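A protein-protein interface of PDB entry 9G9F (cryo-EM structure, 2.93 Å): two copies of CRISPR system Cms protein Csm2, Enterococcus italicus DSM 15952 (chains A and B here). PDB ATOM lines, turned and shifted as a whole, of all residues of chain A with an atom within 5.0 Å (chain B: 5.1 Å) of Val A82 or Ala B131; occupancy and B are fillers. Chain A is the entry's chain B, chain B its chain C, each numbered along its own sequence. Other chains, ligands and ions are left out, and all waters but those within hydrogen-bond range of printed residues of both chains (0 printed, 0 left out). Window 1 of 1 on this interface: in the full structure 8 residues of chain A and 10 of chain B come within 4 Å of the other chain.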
ATOM      1  N   GLU A  78      15.643 -11.576 -21.264  1.00  0.00           N
ATOM      2  CA  GLU A  78      16.946 -12.176 -20.983  1.00  0.00           C
ATOM      3  C   GLU A  78      17.811 -11.221 -20.169  1.00  0.00           C
ATOM      4  O   GLU A  78      18.491 -11.631 -19.216  1.00  0.00           O
ATOM      5  CB  GLU A  78      17.641 -12.562 -22.287  1.00  0.00           C
ATOM      6  CG  GLU A  78      16.980 -13.713 -23.032  1.00  0.00           C
ATOM      7  CD  GLU A  78      17.430 -15.077 -22.539  1.00  0.00           C
ATOM      8  OE1 GLU A  78      17.777 -15.206 -21.346  1.00  0.00           O
ATOM      9  OE2 GLU A  78      17.439 -16.026 -23.351  1.00  0.00           O
ATOM     10  N   TYR A  79      17.782  -9.937 -20.525  1.00  0.00           N
ATOM     11  CA  TYR A  79      18.435  -8.914 -19.721  1.00  0.00           C
ATOM     12  C   TYR A  79      17.900  -8.898 -18.298  1.00  0.00           C
ATOM     13  O   TYR A  79      18.662  -8.706 -17.347  1.00  0.00           O
ATOM     14  CB  TYR A  79      18.236  -7.550 -20.379  1.00  0.00           C
ATOM     15  CG  TYR A  79      18.814  -6.388 -19.611  1.00  0.00           C
ATOM     16  CD1 TYR A  79      20.112  -5.969 -19.832  1.00  0.00           C
ATOM     17  CD2 TYR A  79      18.055  -5.706 -18.671  1.00  0.00           C
ATOM     18  CE1 TYR A  79      20.636  -4.907 -19.142  1.00  0.00           C
ATOM     19  CE2 TYR A  79      18.578  -4.646 -17.970  1.00  0.00           C
ATOM     20  CZ  TYR A  79      19.872  -4.251 -18.209  1.00  0.00           C
ATOM     21  OH  TYR A  79      20.408  -3.190 -17.519  1.00  0.00           O
ATOM     22  N   LEU A  80      16.589  -9.073 -18.139  1.00  0.00           N
ATOM     23  CA  LEU A  80      15.983  -9.090 -16.813  1.00  0.00           C
ATOM     24  C   LEU A  80      16.484 -10.270 -15.994  1.00  0.00           C
ATOM     25  O   LEU A  80      16.728 -10.145 -14.791  1.00  0.00           O
ATOM     26  CB  LEU A  80      14.462  -9.127 -16.948  1.00  0.00           C
ATOM     27  CG  LEU A  80      13.661  -9.645 -15.757  1.00  0.00           C
ATOM     28  CD1 LEU A  80      13.661  -8.623 -14.640  1.00  0.00           C
ATOM     29  CD2 LEU A  80      12.248  -9.984 -16.188  1.00  0.00           C
ATOM     30  N   LYS A  81      16.633 -11.431 -16.632  1.00  0.00           N
ATOM     31  CA  LYS A  81      17.206 -12.585 -15.946  1.00  0.00           C
ATOM     32  C   LYS A  81      18.638 -12.308 -15.510  1.00  0.00           C
ATOM     33  O   LYS A  81      19.043 -12.660 -14.392  1.00  0.00           O
ATOM     34  CB  LYS A  81      17.154 -13.810 -16.856  1.00  0.00           C
ATOM     35  CG  LYS A  81      17.751 -15.061 -16.247  1.00  0.00           C
ATOM     36  CD  LYS A  81      17.763 -16.193 -17.255  1.00  0.00           C
ATOM     37  CE  LYS A  81      16.380 -16.418 -17.843  1.00  0.00           C
ATOM     38  NZ  LYS A  81      16.398 -17.450 -18.912  1.00  0.00           N
ATOM     39  N   VAL A  82      19.423 -11.677 -16.385  1.00  0.00           N
ATOM     40  CA  VAL A  82      20.798 -11.333 -16.029  1.00  0.00           C
ATOM     41  C   VAL A  82      20.819 -10.357 -14.858  1.00  0.00           C
ATOM     42  O   VAL A  82      21.651 -10.468 -13.951  1.00  0.00           O
ATOM     43  CB  VAL A  82      21.541 -10.774 -17.254  1.00  0.00           C
ATOM     44  CG1 VAL A  82      22.825 -10.087 -16.833  1.00  0.00           C
ATOM     45  CG2 VAL A  82      21.847 -11.899 -18.215  1.00  0.00           C
ATOM     46  N   LYS A  83      19.903  -9.390 -14.860  1.00  0.00           N
ATOM     47  CA  LYS A  83      19.821  -8.442 -13.754  1.00  0.00           C
ATOM     48  C   LYS A  83      19.419  -9.140 -12.463  1.00  0.00           C
ATOM     49  O   LYS A  83      19.906  -8.789 -11.384  1.00  0.00           O
ATOM     50  CB  LYS A  83      18.836  -7.328 -14.091  1.00  0.00           C
ATOM     51  CG  LYS A  83      18.927  -6.136 -13.164  1.00  0.00           C
ATOM     52  CD  LYS A  83      20.224  -5.389 -13.402  1.00  0.00           C
ATOM     53  CE  LYS A  83      20.330  -4.950 -14.848  1.00  0.00           C
ATOM     54  NZ  LYS A  83      21.657  -4.364 -15.159  1.00  0.00           N
ATOM     55  N   PHE A  84      18.515 -10.116 -12.554  1.00  0.00           N
ATOM     56  CA  PHE A  84      18.157 -10.913 -11.386  1.00  0.00           C
ATOM     57  C   PHE A  84      19.377 -11.615 -10.815  1.00  0.00           C
ATOM     58  O   PHE A  84      19.597 -11.605  -9.599  1.00  0.00           O
ATOM     59  CB  PHE A  84      17.094 -11.944 -11.760  1.00  0.00           C
ATOM     60  CG  PHE A  84      15.698 -11.419 -11.711  1.00  0.00           C
ATOM     61  CD1 PHE A  84      15.354 -10.416 -10.829  1.00  0.00           C
ATOM     62  CD2 PHE A  84      14.728 -11.933 -12.548  1.00  0.00           C
ATOM     63  CE1 PHE A  84      14.067  -9.934 -10.784  1.00  0.00           C
ATOM     64  CE2 PHE A  84      13.442 -11.457 -12.507  1.00  0.00           C
ATOM     65  CZ  PHE A  84      13.111 -10.456 -11.627  1.00  0.00           C
ATOM     66  N   ALA A  85      20.178 -12.233 -11.683  1.00  0.00           N
ATOM     67  CA  ALA A  85      21.386 -12.906 -11.216  1.00  0.00           C
ATOM     68  C   ALA A  85      22.360 -11.919 -10.589  1.00  0.00           C
ATOM     69  O   ALA A  85      22.988 -12.216  -9.564  1.00  0.00           O
ATOM     70  CB  ALA A  85      22.050 -13.651 -12.367  1.00  0.00           C
ATOM     71  N   TYR A  86      22.503 -10.738 -11.194  1.00  0.00           N
ATOM     72  CA  TYR A  86      23.377  -9.718 -10.624  1.00  0.00           C
ATOM     73  C   TYR A  86      22.905  -9.316  -9.237  1.00  0.00           C
ATOM     74  O   TYR A  86      23.707  -9.206  -8.303  1.00  0.00           O
ATOM     75  CB  TYR A  86      23.437  -8.500 -11.546  1.00  0.00           C
ATOM     76  CG  TYR A  86      24.392  -7.427 -11.076  1.00  0.00           C
ATOM     77  CD1 TYR A  86      25.757  -7.555 -11.272  1.00  0.00           C
ATOM     78  CD2 TYR A  86      23.928  -6.283 -10.445  1.00  0.00           C
ATOM     79  CE1 TYR A  86      26.633  -6.581 -10.849  1.00  0.00           C
ATOM     80  CE2 TYR A  86      24.800  -5.302 -10.017  1.00  0.00           C
ATOM     81  CZ  TYR A  86      26.152  -5.459 -10.222  1.00  0.00           C
ATOM     82  OH  TYR A  86      27.031  -4.492  -9.804  1.00  0.00           O
ATOM     83  N   LEU B  14      23.617 -14.112 -23.832  1.00  0.00           N
ATOM     84  CA  LEU B  14      23.807 -13.911 -22.399  1.00  0.00           C
ATOM     85  C   LEU B  14      23.854 -15.245 -21.659  1.00  0.00           C
ATOM     86  O   LEU B  14      24.655 -15.423 -20.729  1.00  0.00           O
ATOM     87  CB  LEU B  14      22.702 -13.004 -21.851  1.00  0.00           C
ATOM     88  CG  LEU B  14      22.730 -11.504 -22.204  1.00  0.00           C
ATOM     89  CD1 LEU B  14      22.677 -11.218 -23.699  1.00  0.00           C
ATOM     90  CD2 LEU B  14      21.600 -10.765 -21.515  1.00  0.00           C
ATOM     91  N   PHE B 126      28.565  -8.019 -22.498  1.00  0.00           N
ATOM     92  CA  PHE B 126      29.601  -7.766 -21.500  1.00  0.00           C
ATOM     93  C   PHE B 126      28.990  -7.594 -20.112  1.00  0.00           C
ATOM     94  O   PHE B 126      29.585  -8.010 -19.107  1.00  0.00           O
ATOM     95  CB  PHE B 126      30.425  -6.544 -21.891  1.00  0.00           C
ATOM     96  CG  PHE B 126      31.873  -6.650 -21.512  1.00  0.00           C
ATOM     97  CD1 PHE B 126      32.262  -6.591 -20.187  1.00  0.00           C
ATOM     98  CD2 PHE B 126      32.845  -6.820 -22.482  1.00  0.00           C
ATOM     99  CE1 PHE B 126      33.592  -6.691 -19.836  1.00  0.00           C
ATOM    100  CE2 PHE B 126      34.175  -6.921 -22.135  1.00  0.00           C
ATOM    101  CZ  PHE B 126      34.548  -6.855 -20.810  1.00  0.00           C
ATOM    102  N   GLU B 127      27.801  -6.989 -20.044  1.00  0.00           N
ATOM    103  CA  GLU B 127      27.047  -6.960 -18.795  1.00  0.00           C
ATOM    104  C   GLU B 127      26.792  -8.361 -18.275  1.00  0.00           C
ATOM    105  O   GLU B 127      26.931  -8.622 -17.077  1.00  0.00           O
ATOM    106  CB  GLU B 127      25.698  -6.283 -18.984  1.00  0.00           C
ATOM    107  CG  GLU B 127      25.626  -4.805 -18.795  1.00  0.00           C
ATOM    108  CD  GLU B 127      24.185  -4.412 -18.633  1.00  0.00           C
ATOM    109  OE1 GLU B 127      23.858  -3.212 -18.646  1.00  0.00           O
ATOM    110  OE2 GLU B 127      23.374  -5.333 -18.455  1.00  0.00           O
ATOM    111  N   ALA B 128      26.351  -9.258 -19.155  1.00  0.00           N
ATOM    112  CA  ALA B 128      26.077 -10.624 -18.739  1.00  0.00           C
ATOM    113  C   ALA B 128      27.337 -11.276 -18.203  1.00  0.00           C
ATOM    114  O   ALA B 128      27.307 -11.938 -17.163  1.00  0.00           O
ATOM    115  CB  ALA B 128      25.510 -11.427 -19.907  1.00  0.00           C
ATOM    116  N   LEU B 129      28.462 -11.057 -18.881  1.00  0.00           N
ATOM    117  CA  LEU B 129      29.731 -11.599 -18.408  1.00  0.00           C
ATOM    118  C   LEU B 129      30.044 -11.121 -16.994  1.00  0.00           C
ATOM    119  O   LEU B 129      30.291 -11.934 -16.094  1.00  0.00           O
ATOM    120  CB  LEU B 129      30.855 -11.202 -19.362  1.00  0.00           C
ATOM    121  CG  LEU B 129      31.100 -12.113 -20.560  1.00  0.00           C
ATOM    122  CD1 LEU B 129      32.197 -11.529 -21.419  1.00  0.00           C
ATOM    123  CD2 LEU B 129      31.467 -13.507 -20.095  1.00  0.00           C
ATOM    124  N   VAL B 130      30.013  -9.804 -16.769  1.00  0.00           N
ATOM    125  CA  VAL B 130      30.441  -9.284 -15.471  1.00  0.00           C
ATOM    126  C   VAL B 130      29.445  -9.657 -14.377  1.00  0.00           C
ATOM    127  O   VAL B 130      29.837 -10.069 -13.276  1.00  0.00           O
ATOM    128  CB  VAL B 130      30.676  -7.763 -15.538  1.00  0.00           C
ATOM    129  CG1 VAL B 130      29.459  -7.045 -16.076  1.00  0.00           C
ATOM    130  CG2 VAL B 130      31.044  -7.230 -14.164  1.00  0.00           C
ATOM    131  N   ALA B 131      28.145  -9.540 -14.660  1.00  0.00           N
ATOM    132  CA  ALA B 131      27.131  -9.858 -13.662  1.00  0.00           C
ATOM    133  C   ALA B 131      27.161 -11.335 -13.299  1.00  0.00           C
ATOM    134  O   ALA B 131      27.021 -11.701 -12.129  1.00  0.00           O
ATOM    135  CB  ALA B 131      25.750  -9.461 -14.180  1.00  0.00           C
ATOM    136  N   TYR B 132      27.348 -12.203 -14.295  1.00  0.00           N
ATOM    137  CA  TYR B 132      27.361 -13.635 -14.049  1.00  0.00           C
ATOM    138  C   TYR B 132      28.633 -14.058 -13.331  1.00  0.00           C
ATOM    139  O   TYR B 132      28.611 -15.011 -12.545  1.00  0.00           O
ATOM    140  CB  TYR B 132      27.212 -14.357 -15.384  1.00  0.00           C
ATOM    141  CG  TYR B 132      25.778 -14.643 -15.750  1.00  0.00           C
ATOM    142  CD1 TYR B 132      24.789 -14.690 -14.784  1.00  0.00           C
ATOM    143  CD2 TYR B 132      25.398 -14.761 -17.076  1.00  0.00           C
ATOM    144  CE1 TYR B 132      23.476 -14.927 -15.124  1.00  0.00           C
ATOM    145  CE2 TYR B 132      24.083 -14.985 -17.426  1.00  0.00           C
ATOM    146  CZ  TYR B 132      23.128 -15.069 -16.445  1.00  0.00           C
ATOM    147  OH  TYR B 132      21.816 -15.296 -16.792  1.00  0.00           O
ATOM    148  N   ALA B 133      29.747 -13.365 -13.587  1.00  0.00           N
ATOM    149  CA  ALA B 133      30.955 -13.606 -12.808  1.00  0.00           C
ATOM    150  C   ALA B 133      30.767 -13.173 -11.361  1.00  0.00           C
ATOM    151  O   ALA B 133      31.286 -13.814 -10.442  1.00  0.00           O
ATOM    152  CB  ALA B 133      32.140 -12.886 -13.442  1.00  0.00           C
ATOM    153  N   LYS B 134      30.038 -12.076 -11.139  1.00  0.00           N
ATOM    154  CA  LYS B 134      29.719 -11.675  -9.771  1.00  0.00           C
ATOM    155  C   LYS B 134      28.786 -12.680  -9.105  1.00  0.00           C
ATOM    156  O   LYS B 134      28.883 -12.923  -7.897  1.00  0.00           O
ATOM    157  CB  LYS B 134      29.093 -10.282  -9.765  1.00  0.00           C
ATOM    158  CG  LYS B 134      28.885  -9.695  -8.379  1.00  0.00           C
ATOM    159  CD  LYS B 134      30.201  -9.232  -7.784  1.00  0.00           C
ATOM    160  CE  LYS B 134      30.000  -8.564  -6.435  1.00  0.00           C
ATOM    161  NZ  LYS B 134      29.583  -9.534  -5.388  1.00  0.00           N
ATOM    162  N   PHE B 135      27.872 -13.267  -9.881  1.00  0.00           N
ATOM    163  CA  PHE B 135      26.882 -14.187  -9.326  1.00  0.00           C
ATOM    164  C   PHE B 135      27.520 -15.506  -8.905  1.00  0.00           C
ATOM    165  O   PHE B 135      27.265 -16.005  -7.804  1.00  0.00           O
ATOM    166  CB  PHE B 135      25.773 -14.424 -10.350  1.00  0.00           C
ATOM    167  CG  PHE B 135      24.899 -15.605 -10.047  1.00  0.00           C
ATOM    168  CD1 PHE B 135      24.199 -15.680  -8.856  1.00  0.00           C
ATOM    169  CD2 PHE B 135      24.760 -16.629 -10.963  1.00  0.00           C
ATOM    170  CE1 PHE B 135      23.391 -16.762  -8.581  1.00  0.00           C
ATOM    171  CE2 PHE B 135      23.952 -17.711 -10.694  1.00  0.00           C
ATOM    172  CZ  PHE B 135      23.268 -17.778  -9.502  1.00  0.00           C
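O of Glu A78 touches CD2 of Leu B14, at 3.96 Å.
Glu B127 touches Tyr A79 (OE2 to CE1, 2.9 Å).
Val A82 touches Leu B14.
Ala B128 touches Val A82.
CB of Ala B131 touches CG1 of Val A82, at 3.998 Å.
OH of Tyr B132 touches CG2 of Val A82 (3.7 Å).
Tyr B132 touches Ala A85.
Ala A85 touches Phe B135.
Tyr A86 touches Ala B131.
Leu A80 touches none of the printed residues of chain B.
Printed residues of chain B within 4 Å of Val A82: Leu B14 (3.5 Å), Ala B128 (3.8 Å), Ala B131 (3.998 Å) and Tyr B132 (3.7 Å).
Of the printed residues of chain B, Lys A83 touches Glu B127.
Of the printed residues of chain A, Leu B14 touches Glu A78 (3.96 Å) and Val A82 (3.5 Å).
Lys B134 touches none of the printed residues of chain A.
The nearest printed residue of chain A that does not touch Glu B127 is Val A82 (4.4 Å).
The side-chain amino group (NZ) of Lys A83 is in hydrogen-bond range of the side-chain hydroxyl (OH) of Tyr A79, at 2.9 Å.
The side-chain carboxylate (OE1) of Glu A78 lies within salt-bridge range of the side-chain amino group (NZ) of Lys A81, at 3.6 Å.
Of the 9 printed residues of chain A, 6 touch a printed residue of chain B.
Hydrophobic or aromatic side chains of chain B within 4 Å of the printed part of chain A: Leu B14, Ala B131, Tyr B132 and Phe B135.
Among the printed residues, 10 pairs touch across the chains.
No position is printed for both chains.
OE2 of Glu B127 is in salt-bridge range of NZ of Lys A83.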
